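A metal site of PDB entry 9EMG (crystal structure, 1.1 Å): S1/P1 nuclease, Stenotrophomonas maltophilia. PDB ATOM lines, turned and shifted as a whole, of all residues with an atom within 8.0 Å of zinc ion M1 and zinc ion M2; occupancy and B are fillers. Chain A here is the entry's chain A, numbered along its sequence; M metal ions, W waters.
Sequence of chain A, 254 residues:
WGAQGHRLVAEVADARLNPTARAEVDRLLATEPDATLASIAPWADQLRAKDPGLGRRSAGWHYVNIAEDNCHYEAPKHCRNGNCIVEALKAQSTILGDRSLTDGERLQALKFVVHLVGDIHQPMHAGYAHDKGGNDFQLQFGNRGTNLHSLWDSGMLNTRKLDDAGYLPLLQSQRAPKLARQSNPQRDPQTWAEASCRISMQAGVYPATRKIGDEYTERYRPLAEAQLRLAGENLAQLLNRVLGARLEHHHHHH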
ATOM      1  N   TRP A   1     -26.204 -30.581  10.025  1.00  0.00           N
ATOM      2  CA  TRP A   1     -27.084 -31.590   9.406  1.00  0.00           C
ATOM      3  C   TRP A   1     -26.243 -32.619   8.664  1.00  0.00           C
ATOM      4  O   TRP A   1     -25.110 -32.341   8.292  1.00  0.00           O
ATOM      5  CB  TRP A   1     -28.048 -30.947   8.390  1.00  0.00           C
ATOM      6  CG  TRP A   1     -28.884 -29.844   8.945  1.00  0.00           C
ATOM      7  CD1 TRP A   1     -28.637 -28.514   8.852  1.00  0.00           C
ATOM      8  CD2 TRP A   1     -30.100 -29.980   9.693  1.00  0.00           C
ATOM      9  NE1 TRP A   1     -29.615 -27.809   9.463  1.00  0.00           N
ATOM     10  CE2 TRP A   1     -30.553 -28.668   9.976  1.00  0.00           C
ATOM     11  CE3 TRP A   1     -30.902 -31.061  10.094  1.00  0.00           C
ATOM     12  CZ2 TRP A   1     -31.701 -28.424  10.707  1.00  0.00           C
ATOM     13  CZ3 TRP A   1     -32.064 -30.810  10.787  1.00  0.00           C
ATOM     14  CH2 TRP A   1     -32.466 -29.500  11.064  1.00  0.00           C
ATOM     15  N   GLY A   2     -26.850 -33.760   8.397  1.00  0.00           N
ATOM     16  CA  GLY A   2     -26.349 -34.660   7.363  1.00  0.00           C
ATOM     17  C   GLY A   2     -26.691 -34.158   5.989  1.00  0.00           C
ATOM     18  O   GLY A   2     -27.218 -33.032   5.805  1.00  0.00           O
ATOM     19  N   ALA A   3     -26.359 -34.938   4.983  1.00  0.00           N
ATOM     20  CA  ALA A   3     -26.381 -34.467   3.595  1.00  0.00           C
ATOM     21  C   ALA A   3     -27.791 -34.081   3.156  1.00  0.00           C
ATOM     22  O   ALA A   3     -27.970 -33.021   2.544  1.00  0.00           O
ATOM     23  CB  ALA A   3     -25.800 -35.482   2.669  1.00  0.00           C
ATOM     24  N   GLY A   5     -30.369 -32.986   4.961  1.00  0.00           N
ATOM     25  CA  GLY A   5     -30.785 -31.701   5.537  1.00  0.00           C
ATOM     26  C   GLY A   5     -30.124 -30.564   4.763  1.00  0.00           C
ATOM     27  O   GLY A   5     -30.749 -29.544   4.480  1.00  0.00           O
ATOM     28  N   HIS A   6     -28.836 -30.675   4.464  1.00  0.00           N
ATOM     29  CA  HIS A   6     -28.139 -29.602   3.745  1.00  0.00           C
ATOM     30  C   HIS A   6     -28.756 -29.381   2.362  1.00  0.00           C
ATOM     31  O   HIS A   6     -28.952 -28.212   1.994  1.00  0.00           O
ATOM     32  CB  HIS A   6     -26.634 -29.897   3.636  1.00  0.00           C
ATOM     33  CG  HIS A   6     -25.947 -29.612   4.915  1.00  0.00           C
ATOM     34  ND1 HIS A   6     -25.837 -28.313   5.367  1.00  0.00           N
ATOM     35  CD2 HIS A   6     -25.438 -30.393   5.878  1.00  0.00           C
ATOM     36  CE1 HIS A   6     -25.288 -28.345   6.600  1.00  0.00           C
ATOM     37  NE2 HIS A   6     -25.036 -29.614   6.926  1.00  0.00           N
ATOM     38  N   ALA A  41     -24.431 -28.391  -1.487  1.00  0.00           N
ATOM     39  CA  ALA A  41     -24.774 -28.114  -0.085  1.00  0.00           C
ATOM     40  C   ALA A  41     -24.006 -28.994   0.899  1.00  0.00           C
ATOM     41  O   ALA A  41     -23.615 -28.477   1.967  1.00  0.00           O
ATOM     42  CB  ALA A  41     -26.251 -28.125   0.129  1.00  0.00           C
ATOM     43  N   PRO A  42     -23.820 -30.310   0.668  1.00  0.00           N
ATOM     44  CA  PRO A  42     -23.058 -31.141   1.598  1.00  0.00           C
ATOM     45  C   PRO A  42     -21.543 -31.014   1.504  1.00  0.00           C
ATOM     46  O   PRO A  42     -20.832 -31.643   2.314  1.00  0.00           O
ATOM     47  CB  PRO A  42     -23.498 -32.569   1.257  1.00  0.00           C
ATOM     48  CG  PRO A  42     -24.752 -32.401   0.448  1.00  0.00           C
ATOM     49  CD  PRO A  42     -24.514 -31.130  -0.338  1.00  0.00           C
ATOM     50  N   TRP A  43     -21.037 -30.300   0.496  1.00  0.00           N
ATOM     51  CA  TRP A  43     -19.597 -30.315   0.130  1.00  0.00           C
ATOM     52  C   TRP A  43     -18.698 -30.062   1.328  1.00  0.00           C
ATOM     53  O   TRP A  43     -17.705 -30.792   1.521  1.00  0.00           O
ATOM     54  CB  TRP A  43     -19.357 -29.326  -1.003  1.00  0.00           C
ATOM     55  CG  TRP A  43     -17.927 -29.084  -1.387  1.00  0.00           C
ATOM     56  CD1 TRP A  43     -17.204 -29.729  -2.355  1.00  0.00           C
ATOM     57  CD2 TRP A  43     -17.062 -28.063  -0.872  1.00  0.00           C
ATOM     58  NE1 TRP A  43     -15.961 -29.169  -2.463  1.00  0.00           N
ATOM     59  CE2 TRP A  43     -15.848 -28.140  -1.568  1.00  0.00           C
ATOM     60  CE3 TRP A  43     -17.238 -27.055   0.095  1.00  0.00           C
ATOM     61  CZ2 TRP A  43     -14.800 -27.246  -1.336  1.00  0.00           C
ATOM     62  CZ3 TRP A  43     -16.194 -26.181   0.334  1.00  0.00           C
ATOM     63  CH2 TRP A  43     -15.003 -26.280  -0.366  1.00  0.00           C
ATOM     64  N   ALA A  44     -19.030 -29.097   2.166  1.00  0.00           N
ATOM     65  CA  ALA A  44     -18.109 -28.692   3.251  1.00  0.00           C
ATOM     66  C   ALA A  44     -17.919 -29.838   4.246  1.00  0.00           C
ATOM     67  O   ALA A  44     -16.899 -29.849   4.946  1.00  0.00           O
ATOM     68  CB  ALA A  44     -18.609 -27.464   3.943  1.00  0.00           C
ATOM     69  N   ASP A  45     -18.877 -30.750   4.375  1.00  0.00           N
ATOM     70  CA  ASP A  45     -18.718 -31.934   5.253  1.00  0.00           C
ATOM     71  C   ASP A  45     -17.865 -33.036   4.618  1.00  0.00           C
ATOM     72  O   ASP A  45     -17.499 -33.978   5.328  1.00  0.00           O
ATOM     73  CB  ASP A  45     -20.076 -32.508   5.628  1.00  0.00           C
ATOM     74  CG  ASP A  45     -20.823 -31.794   6.727  1.00  0.00           C
ATOM     75  OD1 ASP A  45     -20.217 -30.924   7.383  1.00  0.00           O
ATOM     76  OD2 ASP A  45     -22.011 -32.111   6.916  1.00  0.00           O
ATOM     77  N   GLN A  46     -17.582 -32.960   3.324  1.00  0.00           N
ATOM     78  CA  GLN A  46     -16.908 -34.041   2.593  1.00  0.00           C
ATOM     79  C   GLN A  46     -15.405 -33.760   2.440  1.00  0.00           C
ATOM     80  O   GLN A  46     -14.741 -34.547   1.800  1.00  0.00           O
ATOM     81  CB  GLN A  46     -17.603 -34.244   1.255  1.00  0.00           C
ATOM     82  CG  GLN A  46     -19.132 -34.216   1.327  1.00  0.00           C
ATOM     83  CD  GLN A  46     -19.782 -35.092   2.376  1.00  0.00           C
ATOM     84  OE1 GLN A  46     -19.330 -36.205   2.648  1.00  0.00           O
ATOM     85  NE2 GLN A  46     -20.902 -34.606   2.941  1.00  0.00           N
ATOM     86  N   SER A  58     -11.132 -25.742   8.230  1.00  0.00           N
ATOM     87  CA  SER A  58     -12.558 -25.378   8.317  1.00  0.00           C
ATOM     88  C   SER A  58     -13.404 -26.286   9.233  1.00  0.00           C
ATOM     89  O   SER A  58     -14.592 -26.064   9.360  1.00  0.00           O
ATOM     90  CB  SER A  58     -13.169 -25.250   6.920  1.00  0.00           C
ATOM     91  OG  SER A  58     -13.195 -26.513   6.285  1.00  0.00           O
ATOM     92  N   ALA A  59     -12.814 -27.304   9.865  1.00  0.00           N
ATOM     93  CA  ALA A  59     -13.604 -28.267  10.676  1.00  0.00           C
ATOM     94  C   ALA A  59     -14.420 -27.528  11.731  1.00  0.00           C
ATOM     95  O   ALA A  59     -15.588 -27.906  11.988  1.00  0.00           O
ATOM     96  CB  ALA A  59     -12.687 -29.288  11.297  1.00  0.00           C
ATOM     97  N   TRP A  61     -15.607 -24.609  11.768  1.00  0.00           N
ATOM     98  CA  TRP A  61     -16.545 -23.610  11.234  1.00  0.00           C
ATOM     99  C   TRP A  61     -17.995 -24.118  11.249  1.00  0.00           C
ATOM    100  O   TRP A  61     -18.880 -23.334  10.944  1.00  0.00           O
ATOM    101  CB  TRP A  61     -16.178 -23.240   9.808  1.00  0.00           C
ATOM    102  CG  TRP A  61     -14.849 -22.602   9.613  1.00  0.00           C
ATOM    103  CD1 TRP A  61     -13.876 -22.358  10.529  1.00  0.00           C
ATOM    104  CD2 TRP A  61     -14.335 -22.206   8.331  1.00  0.00           C
ATOM    105  NE1 TRP A  61     -12.785 -21.803   9.904  1.00  0.00           N
ATOM    106  CE2 TRP A  61     -13.039 -21.689   8.560  1.00  0.00           C
ATOM    107  CE3 TRP A  61     -14.843 -22.229   7.035  1.00  0.00           C
ATOM    108  CZ2 TRP A  61     -12.259 -21.196   7.514  1.00  0.00           C
ATOM    109  CZ3 TRP A  61     -14.082 -21.733   6.002  1.00  0.00           C
ATOM    110  CH2 TRP A  61     -12.800 -21.245   6.248  1.00  0.00           C
ATOM    111  N   HIS A  62     -18.224 -25.403  11.548  1.00  0.00           N
ATOM    112  CA  HIS A  62     -19.584 -25.960  11.453  1.00  0.00           C
ATOM    113  C   HIS A  62     -20.386 -25.743  12.737  1.00  0.00           C
ATOM    114  O   HIS A  62     -21.582 -26.081  12.752  1.00  0.00           O
ATOM    115  CB  HIS A  62     -19.529 -27.428  11.086  1.00  0.00           C
ATOM    116  CG  HIS A  62     -18.900 -27.701   9.772  1.00  0.00           C
ATOM    117  ND1 HIS A  62     -19.550 -28.376   8.761  1.00  0.00           N
ATOM    118  CD2 HIS A  62     -17.659 -27.418   9.326  1.00  0.00           C
ATOM    119  CE1 HIS A  62     -18.705 -28.493   7.737  1.00  0.00           C
ATOM    120  NE2 HIS A  62     -17.550 -27.876   8.045  1.00  0.00           N
ATOM    121  N   TYR A  63     -19.765 -25.241  13.815  1.00  0.00           N
ATOM    122  CA  TYR A  63     -20.349 -25.227  15.184  1.00  0.00           C
ATOM    123  C   TYR A  63     -20.143 -23.892  15.871  1.00  0.00           C
ATOM    124  O   TYR A  63     -19.179 -23.159  15.565  1.00  0.00           O
ATOM    125  CB  TYR A  63     -19.718 -26.293  16.096  1.00  0.00           C
ATOM    126  CG  TYR A  63     -19.408 -27.594  15.410  1.00  0.00           C
ATOM    127  CD1 TYR A  63     -20.394 -28.531  15.200  1.00  0.00           C
ATOM    128  CD2 TYR A  63     -18.160 -27.862  14.895  1.00  0.00           C
ATOM    129  CE1 TYR A  63     -20.142 -29.712  14.533  1.00  0.00           C
ATOM    130  CE2 TYR A  63     -17.880 -29.026  14.224  1.00  0.00           C
ATOM    131  CZ  TYR A  63     -18.872 -29.971  14.041  1.00  0.00           C
ATOM    132  OH  TYR A  63     -18.584 -31.130  13.373  1.00  0.00           O
ATOM    133  N   ILE A  85     -18.824 -21.081  13.594  1.00  0.00           N
ATOM    134  CA  ILE A  85     -19.757 -20.849  12.469  1.00  0.00           C
ATOM    135  C   ILE A  85     -20.188 -19.396  12.362  1.00  0.00           C
ATOM    136  O   ILE A  85     -20.461 -18.969  11.235  1.00  0.00           O
ATOM    137  CB  ILE A  85     -20.966 -21.792  12.582  1.00  0.00           C
ATOM    138  CG1 ILE A  85     -21.766 -21.795  11.272  1.00  0.00           C
ATOM    139  CG2 ILE A  85     -21.842 -21.521  13.793  1.00  0.00           C
ATOM    140  CD1 ILE A  85     -22.567 -23.076  11.118  1.00  0.00           C
ATOM    141  N   HIS A 115     -23.770 -24.223   2.969  1.00  0.00           N
ATOM    142  CA  HIS A 115     -23.645 -25.262   4.022  1.00  0.00           C
ATOM    143  C   HIS A 115     -23.866 -24.665   5.408  1.00  0.00           C
ATOM    144  O   HIS A 115     -24.582 -25.208   6.224  1.00  0.00           O
ATOM    145  CB  HIS A 115     -22.271 -25.918   3.945  1.00  0.00           C
ATOM    146  CG  HIS A 115     -22.128 -27.078   4.865  1.00  0.00           C
ATOM    147  ND1 HIS A 115     -22.498 -28.352   4.467  1.00  0.00           N
ATOM    148  CD2 HIS A 115     -21.746 -27.170   6.152  1.00  0.00           C
ATOM    149  CE1 HIS A 115     -22.272 -29.182   5.494  1.00  0.00           C
ATOM    150  NE2 HIS A 115     -21.826 -28.474   6.528  1.00  0.00           N
ATOM    151  N   LEU A 116     -23.187 -23.537   5.662  1.00  0.00           N
ATOM    152  CA  LEU A 116     -23.166 -22.963   7.006  1.00  0.00           C
ATOM    153  C   LEU A 116     -24.516 -22.347   7.363  1.00  0.00           C
ATOM    154  O   LEU A 116     -24.875 -22.353   8.536  1.00  0.00           O
ATOM    155  CB  LEU A 116     -22.007 -21.978   7.161  1.00  0.00           C
ATOM    156  CG  LEU A 116     -20.618 -22.608   7.041  1.00  0.00           C
ATOM    157  CD1 LEU A 116     -19.539 -21.536   7.192  1.00  0.00           C
ATOM    158  CD2 LEU A 116     -20.383 -23.728   8.038  1.00  0.00           C
ATOM    159  N   GLY A 118     -27.197 -23.699   6.635  1.00  0.00           N
ATOM    160  CA  GLY A 118     -27.845 -24.917   7.137  1.00  0.00           C
ATOM    161  C   GLY A 118     -27.394 -25.240   8.568  1.00  0.00           C
ATOM    162  O   GLY A 118     -28.198 -25.395   9.483  1.00  0.00           O
ATOM    163  N   ASP A 119     -26.082 -25.359   8.762  1.00  0.00           N
ATOM    164  CA  ASP A 119     -25.561 -25.801  10.078  1.00  0.00           C
ATOM    165  C   ASP A 119     -25.935 -24.843  11.201  1.00  0.00           C
ATOM    166  O   ASP A 119     -26.177 -25.289  12.333  1.00  0.00           O
ATOM    167  CB  ASP A 119     -24.052 -26.027  10.052  1.00  0.00           C
ATOM    168  CG  ASP A 119     -23.616 -27.417   9.605  1.00  0.00           C
ATOM    169  OD1 ASP A 119     -24.522 -28.269   9.506  1.00  0.00           O
ATOM    170  OD2 ASP A 119     -22.408 -27.569   9.353  1.00  0.00           O
ATOM    171  N   ILE A 120     -26.009 -23.530  10.941  1.00  0.00           N
ATOM    172  CA  ILE A 120     -26.255 -22.562  12.024  1.00  0.00           C
ATOM    173  C   ILE A 120     -27.719 -22.617  12.461  1.00  0.00           C
ATOM    174  O   ILE A 120     -28.041 -22.012  13.497  1.00  0.00           O
ATOM    175  CB  ILE A 120     -25.774 -21.151  11.604  1.00  0.00           C
ATOM    176  CG1 ILE A 120     -25.442 -20.277  12.804  1.00  0.00           C
ATOM    177  CG2 ILE A 120     -26.769 -20.485  10.672  1.00  0.00           C
ATOM    178  CD1 ILE A 120     -24.699 -19.010  12.427  1.00  0.00           C
ATOM    179  N   GLN A 122     -29.097 -25.766  12.804  1.00  0.00           N
ATOM    180  CA  GLN A 122     -29.171 -27.083  13.472  1.00  0.00           C
ATOM    181  C   GLN A 122     -28.949 -26.876  14.958  1.00  0.00           C
ATOM    182  O   GLN A 122     -27.843 -26.498  15.353  1.00  0.00           O
ATOM    183  CB  GLN A 122     -28.129 -27.989  12.848  1.00  0.00           C
ATOM    184  CG  GLN A 122     -27.889 -29.251  13.649  1.00  0.00           C
ATOM    185  CD  GLN A 122     -29.152 -30.000  14.018  1.00  0.00           C
ATOM    186  OE1 GLN A 122     -29.489 -30.160  15.191  1.00  0.00           O
ATOM    187  NE2 GLN A 122     -29.872 -30.463  13.023  1.00  0.00           N
ATOM    188  N   HIS A 125     -25.700 -28.034  16.517  1.00  0.00           N
ATOM    189  CA  HIS A 125     -24.475 -27.315  16.100  1.00  0.00           C
ATOM    190  C   HIS A 125     -24.287 -26.009  16.880  1.00  0.00           C
ATOM    191  O   HIS A 125     -23.319 -25.305  16.604  1.00  0.00           O
ATOM    192  CB  HIS A 125     -24.470 -27.079  14.590  1.00  0.00           C
ATOM    193  CG  HIS A 125     -24.127 -28.297  13.793  1.00  0.00           C
ATOM    194  ND1 HIS A 125     -23.147 -28.285  12.830  1.00  0.00           N
ATOM    195  CD2 HIS A 125     -24.590 -29.587  13.833  1.00  0.00           C
ATOM    196  CE1 HIS A 125     -23.009 -29.513  12.345  1.00  0.00           C
ATOM    197  NE2 HIS A 125     -23.907 -30.324  12.910  1.00  0.00           N
ATOM    198  N   HIS A 149     -26.747 -35.848  18.837  1.00  0.00           N
ATOM    199  CA  HIS A 149     -26.291 -35.037  17.699  1.00  0.00           C
ATOM    200  C   HIS A 149     -26.789 -35.628  16.382  1.00  0.00           C
ATOM    201  O   HIS A 149     -27.420 -34.926  15.573  1.00  0.00           O
ATOM    202  CB  HIS A 149     -24.782 -34.854  17.765  1.00  0.00           C
ATOM    203  CG  HIS A 149     -24.299 -33.883  16.744  1.00  0.00           C
ATOM    204  ND1 HIS A 149     -24.008 -32.568  17.071  1.00  0.00           N
ATOM    205  CD2 HIS A 149     -24.123 -33.996  15.398  1.00  0.00           C
ATOM    206  CE1 HIS A 149     -23.652 -31.937  15.945  1.00  0.00           C
ATOM    207  NE2 HIS A 149     -23.704 -32.759  14.909  1.00  0.00           N
ATOM    208  N   ASP A 153     -29.199 -34.288  13.418  1.00  0.00           N
ATOM    209  CA  ASP A 153     -28.630 -34.089  12.076  1.00  0.00           C
ATOM    210  C   ASP A 153     -29.401 -34.876  11.005  1.00  0.00           C
ATOM    211  O   ASP A 153     -29.521 -34.385   9.853  1.00  0.00           O
ATOM    212  CB  ASP A 153     -27.163 -34.447  11.999  1.00  0.00           C
ATOM    213  CG  ASP A 153     -26.171 -33.338  12.333  1.00  0.00           C
ATOM    214  OD1 ASP A 153     -26.575 -32.208  12.583  1.00  0.00           O
ATOM    215  OD2 ASP A 153     -24.972 -33.667  12.264  1.00  0.00           O
HETATM  216 ZN    ZN M   1     -24.497 -30.232   8.801  1.00  0.00          ZN
HETATM  217 ZN    ZN M   2     -21.403 -29.179   8.451  1.00  0.00          ZN
HETATM  218 ZN    ZN M   3     -23.698 -32.338  12.937  1.00  0.00          ZN
HETATM  219  O   HOH W   1     -22.606 -30.547   9.125  1.00  0.00           O
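Zinc ion M1 is bound by water W1 (1.9 Å), a ring nitrogen (NE2) of His 6 (2.0 Å), the side-chain carboxylate of Asp 119 (2.1 Å), the backbone nitrogen of Trp 1 (2.1 Å) and the backbone carbonyl oxygen of Trp 1 (2.3 Å). Zinc ion M1 has five donor atoms within binding distance.
Within 4 Å of zinc ion M2: His 6, Asp 45, His 62, His 115 and Asp 119. The nearest printed residue that does not touch zinc ion M2 is His 125 (4.2 Å).
A ring nitrogen (ND1) of His 125 lies within hydrogen-bond range of the backbone carbonyl oxygen (O) of His 62 (2.7 Å). ND1 of His 6 sits close to O of His 115 (3.5 Å). A ring nitrogen (ND1) of His 115 is in hydrogen-bond range of the backbone carbonyl oxygen (O) of Ala 41, at 2.7 Å. The side-chain carboxylate (OD1) of Asp 153 lies close to the backbone NH (N) of Trp 1. The backbone carbonyl oxygen (O) of Gly 118 sits at hydrogen-bond distance from the indole nitrogen (NE1) of Trp 1.
Zinc ion M2 is bound by water W1, a ring nitrogen (ND1) of His 62, a ring nitrogen (NE2) of His 115, the side-chain carboxylate of Asp 119 and the side-chain carboxylate of Asp 45.
His 125 touches zinc ion M1 (CE1 to ZN, 3.9 Å). Of the 26 residues printed, 6 come within 4 Å of zinc ion M1.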
